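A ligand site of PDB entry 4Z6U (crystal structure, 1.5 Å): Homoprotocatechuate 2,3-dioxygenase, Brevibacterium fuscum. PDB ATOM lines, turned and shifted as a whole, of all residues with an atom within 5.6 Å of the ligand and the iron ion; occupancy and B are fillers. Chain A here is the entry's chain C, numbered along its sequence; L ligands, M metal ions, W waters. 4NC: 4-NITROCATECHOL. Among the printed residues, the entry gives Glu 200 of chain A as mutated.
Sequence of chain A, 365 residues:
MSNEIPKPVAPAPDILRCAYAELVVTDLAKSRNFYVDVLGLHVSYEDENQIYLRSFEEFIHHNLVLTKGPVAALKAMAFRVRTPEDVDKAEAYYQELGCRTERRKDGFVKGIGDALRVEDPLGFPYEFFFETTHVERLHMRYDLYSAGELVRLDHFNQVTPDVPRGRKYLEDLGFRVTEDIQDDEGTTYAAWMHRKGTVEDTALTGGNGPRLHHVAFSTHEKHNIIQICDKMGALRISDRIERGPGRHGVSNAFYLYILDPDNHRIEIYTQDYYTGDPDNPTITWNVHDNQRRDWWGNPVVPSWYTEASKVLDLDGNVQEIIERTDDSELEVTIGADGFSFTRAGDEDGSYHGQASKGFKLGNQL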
ATOM      1  N   HIS A 155      12.290  -1.653   2.093  1.00  0.00           N
ATOM      2  CA  HIS A 155      12.001  -0.515   1.209  1.00  0.00           C
ATOM      3  C   HIS A 155      10.753   0.231   1.629  1.00  0.00           C
ATOM      4  O   HIS A 155       9.973  -0.254   2.454  1.00  0.00           O
ATOM      5  CB  HIS A 155      11.861  -0.997  -0.253  1.00  0.00           C
ATOM      6  CG  HIS A 155      10.708  -1.901  -0.523  1.00  0.00           C
ATOM      7  ND1 HIS A 155      10.803  -3.274  -0.589  1.00  0.00           N
ATOM      8  CD2 HIS A 155       9.429  -1.606  -0.818  1.00  0.00           C
ATOM      9  CE1 HIS A 155       9.629  -3.789  -0.894  1.00  0.00           C
ATOM     10  NE2 HIS A 155       8.781  -2.794  -1.042  1.00  0.00           N
ATOM     11  N   ASN A 157       7.421   2.398  -0.459  1.00  0.00           N
ATOM     12  CA  ASN A 157       6.746   2.552  -1.738  1.00  0.00           C
ATOM     13  C   ASN A 157       5.833   3.767  -1.615  1.00  0.00           C
ATOM     14  O   ASN A 157       5.020   3.869  -0.694  1.00  0.00           O
ATOM     15  CB  ASN A 157       6.009   1.283  -2.169  1.00  0.00           C
ATOM     16  CG  ASN A 157       5.387   1.383  -3.545  1.00  0.00           C
ATOM     17  OD1 ASN A 157       4.641   2.325  -3.862  1.00  0.00           O
ATOM     18  ND2 ASN A 157       5.692   0.411  -4.397  1.00  0.00           N
ATOM     19  N   ILE A 181       6.894  -0.587 -14.973  1.00  0.00           N
ATOM     20  CA  ILE A 181       5.727  -1.026 -15.688  1.00  0.00           C
ATOM     21  C   ILE A 181       5.274   0.118 -16.621  1.00  0.00           C
ATOM     22  O   ILE A 181       5.064   1.270 -16.169  1.00  0.00           O
ATOM     23  CB  ILE A 181       4.552  -1.413 -14.744  1.00  0.00           C
ATOM     24  CG1 ILE A 181       4.937  -2.597 -13.848  1.00  0.00           C
ATOM     25  CG2 ILE A 181       3.301  -1.711 -15.529  1.00  0.00           C
ATOM     26  CD1 ILE A 181       3.935  -2.888 -12.732  1.00  0.00           C
ATOM     27  N   TRP A 192      10.739   1.052  -9.781  1.00  0.00           N
ATOM     28  CA  TRP A 192      11.430   0.595  -8.582  1.00  0.00           C
ATOM     29  C   TRP A 192      12.904   0.987  -8.692  1.00  0.00           C
ATOM     30  O   TRP A 192      13.462   0.922  -9.750  1.00  0.00           O
ATOM     31  CB  TRP A 192      11.354  -0.933  -8.495  1.00  0.00           C
ATOM     32  CG  TRP A 192       9.991  -1.454  -8.096  1.00  0.00           C
ATOM     33  CD1 TRP A 192       9.668  -1.940  -6.868  1.00  0.00           C
ATOM     34  CD2 TRP A 192       8.805  -1.599  -8.917  1.00  0.00           C
ATOM     35  NE1 TRP A 192       8.345  -2.337  -6.848  1.00  0.00           N
ATOM     36  CE2 TRP A 192       7.793  -2.132  -8.085  1.00  0.00           C
ATOM     37  CE3 TRP A 192       8.473  -1.254 -10.252  1.00  0.00           C
ATOM     38  CZ2 TRP A 192       6.499  -2.398  -8.554  1.00  0.00           C
ATOM     39  CZ3 TRP A 192       7.183  -1.534 -10.722  1.00  0.00           C
ATOM     40  CH2 TRP A 192       6.209  -2.110  -9.882  1.00  0.00           C
ATOM     41  N   GLU A 200      14.946  -2.608  -4.662  1.00  0.00           N
ATOM     42  CA  GLU A 200      14.385  -1.313  -4.268  1.00  0.00           C
ATOM     43  C   GLU A 200      14.819  -0.883  -2.861  1.00  0.00           C
ATOM     44  O   GLU A 200      14.935  -1.690  -1.944  1.00  0.00           O
ATOM     45  CB  GLU A 200      12.855  -1.356  -4.328  1.00  0.00           C
ATOM     46  CG  GLU A 200      12.298  -2.686  -3.777  1.00  0.00           C
ATOM     47  CD  GLU A 200      10.796  -2.800  -3.861  1.00  0.00           C
ATOM     48  OE1 GLU A 200      10.114  -1.716  -3.775  1.00  0.00           O
ATOM     49  OE2 GLU A 200      10.304  -3.976  -4.012  1.00  0.00           O
ATOM     50  N   HIS A 214       3.296   1.755   1.102  1.00  0.00           N
ATOM     51  CA  HIS A 214       3.659   0.802   2.137  1.00  0.00           C
ATOM     52  C   HIS A 214       5.088   0.938   2.600  1.00  0.00           C
ATOM     53  O   HIS A 214       5.896   1.615   1.974  1.00  0.00           O
ATOM     54  CB  HIS A 214       3.401  -0.642   1.678  1.00  0.00           C
ATOM     55  CG  HIS A 214       4.185  -1.092   0.490  1.00  0.00           C
ATOM     56  ND1 HIS A 214       3.658  -1.052  -0.782  1.00  0.00           N
ATOM     57  CD2 HIS A 214       5.409  -1.635   0.375  1.00  0.00           C
ATOM     58  CE1 HIS A 214       4.532  -1.590  -1.626  1.00  0.00           C
ATOM     59  NE2 HIS A 214       5.611  -1.934  -0.948  1.00  0.00           N
ATOM     60  N   ALA A 216       8.077  -1.911   3.679  1.00  0.00           N
ATOM     61  CA  ALA A 216       8.324  -3.353   3.517  1.00  0.00           C
ATOM     62  C   ALA A 216       9.446  -3.842   4.409  1.00  0.00           C
ATOM     63  O   ALA A 216      10.510  -3.222   4.463  1.00  0.00           O
ATOM     64  CB  ALA A 216       8.676  -3.677   2.074  1.00  0.00           C
ATOM     65  N   ARG A 243      -3.687  -8.541   0.489  1.00  0.00           N
ATOM     66  CA  ARG A 243      -3.297  -9.106  -0.816  1.00  0.00           C
ATOM     67  C   ARG A 243      -2.146 -10.073  -0.596  1.00  0.00           C
ATOM     68  O   ARG A 243      -1.233  -9.797   0.147  1.00  0.00           O
ATOM     69  CB  ARG A 243      -2.865  -7.989  -1.757  1.00  0.00           C
ATOM     70  CG  ARG A 243      -2.224  -8.453  -3.053  1.00  0.00           C
ATOM     71  CD  ARG A 243      -2.012  -7.361  -4.078  1.00  0.00           C
ATOM     72  NE  ARG A 243      -1.146  -7.922  -5.097  1.00  0.00           N
ATOM     73  CZ  ARG A 243      -0.065  -7.374  -5.663  1.00  0.00           C
ATOM     74  NH1 ARG A 243       0.254  -6.090  -5.500  1.00  0.00           N
ATOM     75  NH2 ARG A 243       0.709  -8.135  -6.404  1.00  0.00           N
ATOM     76  N   HIS A 248       5.837 -12.047  -6.678  1.00  0.00           N
ATOM     77  CA  HIS A 248       5.778 -10.889  -7.577  1.00  0.00           C
ATOM     78  C   HIS A 248       6.381 -11.233  -8.933  1.00  0.00           C
ATOM     79  O   HIS A 248       7.313 -12.033  -9.033  1.00  0.00           O
ATOM     80  CB  HIS A 248       6.612  -9.746  -7.029  1.00  0.00           C
ATOM     81  CG  HIS A 248       5.998  -8.927  -5.950  1.00  0.00           C
ATOM     82  ND1 HIS A 248       4.727  -8.388  -6.014  1.00  0.00           N
ATOM     83  CD2 HIS A 248       6.543  -8.493  -4.771  1.00  0.00           C
ATOM     84  CE1 HIS A 248       4.513  -7.669  -4.921  1.00  0.00           C
ATOM     85  NE2 HIS A 248       5.597  -7.714  -4.158  1.00  0.00           N
ATOM     86  N   GLY A 249       5.882 -10.576  -9.976  1.00  0.00           N
ATOM     87  CA  GLY A 249       6.601 -10.511 -11.253  1.00  0.00           C
ATOM     88  C   GLY A 249       7.767  -9.549 -11.136  1.00  0.00           C
ATOM     89  O   GLY A 249       8.929  -9.949 -11.003  1.00  0.00           O
ATOM     90  N   VAL A 250       7.428  -8.251 -11.128  1.00  0.00           N
ATOM     91  CA  VAL A 250       8.408  -7.231 -10.743  1.00  0.00           C
ATOM     92  C   VAL A 250       9.034  -7.612  -9.381  1.00  0.00           C
ATOM     93  O   VAL A 250       8.330  -7.774  -8.401  1.00  0.00           O
ATOM     94  CB  VAL A 250       7.744  -5.851 -10.607  1.00  0.00           C
ATOM     95  CG1 VAL A 250       8.743  -4.842 -10.037  1.00  0.00           C
ATOM     96  CG2 VAL A 250       7.197  -5.369 -11.945  1.00  0.00           C
ATOM     97  N   SER A 251      10.349  -7.741  -9.364  1.00  0.00           N
ATOM     98  CA  SER A 251      11.229  -8.026  -8.192  1.00  0.00           C
ATOM     99  C   SER A 251      11.452  -9.504  -7.962  1.00  0.00           C
ATOM    100  O   SER A 251      12.449  -9.861  -7.324  1.00  0.00           O
ATOM    101  CB  SER A 251      10.753  -7.386  -6.868  1.00  0.00           C
ATOM    102  OG  SER A 251       9.724  -8.166  -6.256  1.00  0.00           O
ATOM    103  N   TYR A 257       0.845  -8.423   1.678  1.00  0.00           N
ATOM    104  CA  TYR A 257       0.457  -7.116   2.191  1.00  0.00           C
ATOM    105  C   TYR A 257      -0.607  -7.207   3.265  1.00  0.00           C
ATOM    106  O   TYR A 257      -1.670  -7.822   3.050  1.00  0.00           O
ATOM    107  CB  TYR A 257      -0.105  -6.232   1.051  1.00  0.00           C
ATOM    108  CG  TYR A 257       0.874  -5.989  -0.057  1.00  0.00           C
ATOM    109  CD1 TYR A 257       1.796  -4.942   0.002  1.00  0.00           C
ATOM    110  CD2 TYR A 257       0.867  -6.787  -1.186  1.00  0.00           C
ATOM    111  CE1 TYR A 257       2.685  -4.707  -1.046  1.00  0.00           C
ATOM    112  CE2 TYR A 257       1.759  -6.566  -2.235  1.00  0.00           C
ATOM    113  CZ  TYR A 257       2.663  -5.554  -2.144  1.00  0.00           C
ATOM    114  OH  TYR A 257       3.509  -5.334  -3.215  1.00  0.00           O
ATOM    115  N   GLU A 267       4.269  -4.403   3.774  1.00  0.00           N
ATOM    116  CA  GLU A 267       4.608  -5.519   2.905  1.00  0.00           C
ATOM    117  C   GLU A 267       5.628  -6.386   3.638  1.00  0.00           C
ATOM    118  O   GLU A 267       6.555  -5.875   4.277  1.00  0.00           O
ATOM    119  CB  GLU A 267       5.178  -5.059   1.543  1.00  0.00           C
ATOM    120  CG  GLU A 267       5.369  -6.249   0.585  1.00  0.00           C
ATOM    121  CD  GLU A 267       5.990  -5.891  -0.721  1.00  0.00           C
ATOM    122  OE1 GLU A 267       6.534  -4.769  -0.859  1.00  0.00           O
ATOM    123  OE2 GLU A 267       5.888  -6.709  -1.659  1.00  0.00           O
ATOM    124  N   TYR A 269       8.310  -9.451   2.559  1.00  0.00           N
ATOM    125  CA  TYR A 269       8.992  -9.612   1.295  1.00  0.00           C
ATOM    126  C   TYR A 269      10.230 -10.495   1.497  1.00  0.00           C
ATOM    127  O   TYR A 269      10.934 -10.391   2.504  1.00  0.00           O
ATOM    128  CB  TYR A 269       9.425  -8.182   0.899  1.00  0.00           C
ATOM    129  CG  TYR A 269      10.124  -7.860  -0.388  1.00  0.00           C
ATOM    130  CD1 TYR A 269       9.398  -7.432  -1.496  1.00  0.00           C
ATOM    131  CD2 TYR A 269      11.510  -7.851  -0.467  1.00  0.00           C
ATOM    132  CE1 TYR A 269      10.021  -7.041  -2.654  1.00  0.00           C
ATOM    133  CE2 TYR A 269      12.143  -7.449  -1.642  1.00  0.00           C
ATOM    134  CZ  TYR A 269      11.388  -7.022  -2.726  1.00  0.00           C
ATOM    135  OH  TYR A 269      12.043  -6.603  -3.883  1.00  0.00           O
ATOM    136  N   ARG A 292       2.674  -9.619 -14.077  1.00  0.00           N
ATOM    137  CA  ARG A 292       3.635  -8.588 -13.702  1.00  0.00           C
ATOM    138  C   ARG A 292       3.661  -8.300 -12.194  1.00  0.00           C
ATOM    139  O   ARG A 292       4.691  -7.984 -11.658  1.00  0.00           O
ATOM    140  CB  ARG A 292       3.360  -7.311 -14.478  1.00  0.00           C
ATOM    141  CG  ARG A 292       2.203  -6.503 -13.957  1.00  0.00           C
ATOM    142  CD  ARG A 292       1.650  -5.457 -14.918  1.00  0.00           C
ATOM    143  NE  ARG A 292       0.528  -4.771 -14.227  1.00  0.00           N
ATOM    144  CZ  ARG A 292      -0.683  -5.303 -14.040  1.00  0.00           C
ATOM    145  NH1 ARG A 292      -0.980  -6.500 -14.515  1.00  0.00           N
ATOM    146  NH2 ARG A 292      -1.596  -4.662 -13.322  1.00  0.00           N
ATOM    147  N   ARG A 293       2.487  -8.352 -11.550  1.00  0.00           N
ATOM    148  CA  ARG A 293       2.366  -7.978 -10.148  1.00  0.00           C
ATOM    149  C   ARG A 293       2.281  -9.228  -9.270  1.00  0.00           C
ATOM    150  O   ARG A 293       3.015  -9.349  -8.274  1.00  0.00           O
ATOM    151  CB  ARG A 293       1.186  -7.023  -9.905  1.00  0.00           C
ATOM    152  CG  ARG A 293       1.510  -5.615 -10.405  1.00  0.00           C
ATOM    153  CD  ARG A 293       0.677  -4.571  -9.729  1.00  0.00           C
ATOM    154  NE  ARG A 293       1.047  -3.199 -10.111  1.00  0.00           N
ATOM    155  CZ  ARG A 293       1.969  -2.445  -9.535  1.00  0.00           C
ATOM    156  NH1 ARG A 293       2.705  -2.900  -8.523  1.00  0.00           N
ATOM    157  NH2 ARG A 293       2.177  -1.240  -9.967  1.00  0.00           N
ATOM    158  N   ASP A 294       1.410 -10.147  -9.638  1.00  0.00           N
ATOM    159  CA  ASP A 294       1.404 -11.479  -9.081  1.00  0.00           C
ATOM    160  C   ASP A 294       1.744 -12.423 -10.216  1.00  0.00           C
ATOM    161  O   ASP A 294       1.000 -12.516 -11.186  1.00  0.00           O
ATOM    162  CB  ASP A 294       0.059 -11.837  -8.496  1.00  0.00           C
ATOM    163  CG  ASP A 294       0.110 -13.117  -7.716  1.00  0.00           C
ATOM    164  OD1 ASP A 294       0.561 -13.079  -6.529  1.00  0.00           O
ATOM    165  OD2 ASP A 294      -0.272 -14.150  -8.299  1.00  0.00           O
ATOM    166  N   TRP A 304      -5.759  -2.071  -3.245  1.00  0.00           N
ATOM    167  CA  TRP A 304      -4.291  -1.993  -3.349  1.00  0.00           C
ATOM    168  C   TRP A 304      -3.880  -0.813  -4.221  1.00  0.00           C
ATOM    169  O   TRP A 304      -2.881  -0.151  -3.943  1.00  0.00           O
ATOM    170  CB  TRP A 304      -3.732  -3.323  -3.856  1.00  0.00           C
ATOM    171  CG  TRP A 304      -2.237  -3.452  -3.639  1.00  0.00           C
ATOM    172  CD1 TRP A 304      -1.624  -3.953  -2.530  1.00  0.00           C
ATOM    173  CD2 TRP A 304      -1.201  -2.977  -4.493  1.00  0.00           C
ATOM    174  NE1 TRP A 304      -0.280  -3.883  -2.666  1.00  0.00           N
ATOM    175  CE2 TRP A 304       0.029  -3.266  -3.849  1.00  0.00           C
ATOM    176  CE3 TRP A 304      -1.176  -2.355  -5.745  1.00  0.00           C
ATOM    177  CZ2 TRP A 304       1.250  -2.951  -4.388  1.00  0.00           C
ATOM    178  CZ3 TRP A 304       0.050  -2.005  -6.265  1.00  0.00           C
ATOM    179  CH2 TRP A 304       1.256  -2.322  -5.599  1.00  0.00           C
HETATM  180  C1  4NC L   1       7.206  -4.693  -4.676  1.00  0.00           C
HETATM  181  C2  4NC L   1       5.765  -4.276  -4.629  1.00  0.00           C
HETATM  182  C3  4NC L   1       4.925  -4.467  -5.721  1.00  0.00           C
HETATM  183  C4  4NC L   1       5.444  -5.188  -6.826  1.00  0.00           C
HETATM  184  C5  4NC L   1       6.775  -5.622  -6.837  1.00  0.00           C
HETATM  185  C6  4NC L   1       7.658  -5.393  -5.760  1.00  0.00           C
HETATM  186  O7  4NC L   1       7.876  -4.484  -3.522  1.00  0.00           O
HETATM  187  O8  4NC L   1       5.343  -3.720  -3.487  1.00  0.00           O
HETATM  188  N9  4NC L   1       4.517  -5.685  -7.747  1.00  0.00           N
HETATM  189  O10 4NC L   1       4.949  -6.527  -8.720  1.00  0.00           O
HETATM  190  O11 4NC L   1       3.006  -5.708  -7.349  1.00  0.00           O
HETATM  191 FE    FE M   1       6.897  -3.203  -2.182  1.00  0.00          FE
HETATM  192  O   HOH W   1       7.400  -1.711  -3.670  1.00  0.00           O
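The side-chain hydroxyl of Tyr 257 lies close to an oxygen (O8) of the ligand (2.5 Å).
O11 of the ligand lies within hydrogen-bond range of NH1 of Arg 293, at 3.1 Å.
NH1 of Arg 243 is in hydrogen-bond range of O11 of the ligand.
A ring nitrogen (ND1) of His 248 lies within hydrogen-bond range of an oxygen (O10) of the ligand.
OE2 of Glu 200 lies close to O7 of the ligand (2.5 Å).
OE1 of Glu 267 binds the iron ion (2.1 Å).
The iron ion is bound by O8 of the ligand, at 2.1 Å.
An oxygen (O7) of the ligand binds the iron ion (2.1 Å).
The iron ion is bound by water W1, at 2.2 Å.
The iron ion is bound by NE2 of His 214 (2.2 Å).
The iron ion is bound by NE2 of His 155 (2.2 Å).
O of Arg 292 sits close to O10 of the ligand, at 3.3 Å.
Trp 192 touches the ligand.
Val 250 touches the ligand (O to C5, 3.1 Å).
Ser 251 touches the ligand (OG to C6, 3.5 Å).
Tyr 269 touches the ligand.
Of the 19 residues printed, 13 come within 4 Å of the ligand.
The nearest printed residue that does not touch the ligand is Trp 304 (4.2 Å).
OE1 of Glu 200 touches the iron ion (3.9 Å).
Water W1 lies within hydrogen-bond range of the side-chain carboxylate (OE1) of Glu 200, the side-chain amide nitrogen (ND2) of Asn 157 and the indole nitrogen (NE1) of Trp 192.
A ring nitrogen (NE2) of His 248 sits close to the side-chain hydroxyl of Tyr 257 (3.3 Å).
The backbone carbonyl oxygen (O) of Arg 293 sits at hydrogen-bond distance from a ring nitrogen (ND1) of His 248 (3.0 Å).
The guanidinium group (NH2) of Arg 243 sits at hydrogen-bond distance from the backbone carbonyl oxygen (O) of Arg 293.
OH of Tyr 257 lies within hydrogen-bond range of OE2 of Glu 267, at 3.2 Å.
OE2 of Glu 200 is in hydrogen-bond range of OH of Tyr 269, at 3.2 Å.
OE1 of Glu 200 lies close to NE2 of His 155 (3.2 Å).
O of Arg 292 sits close to N of Gly 249 (3.3 Å).
The backbone carbonyl oxygen (O) of Arg 292 sits at hydrogen-bond distance from the backbone NH (N) of Val 250.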
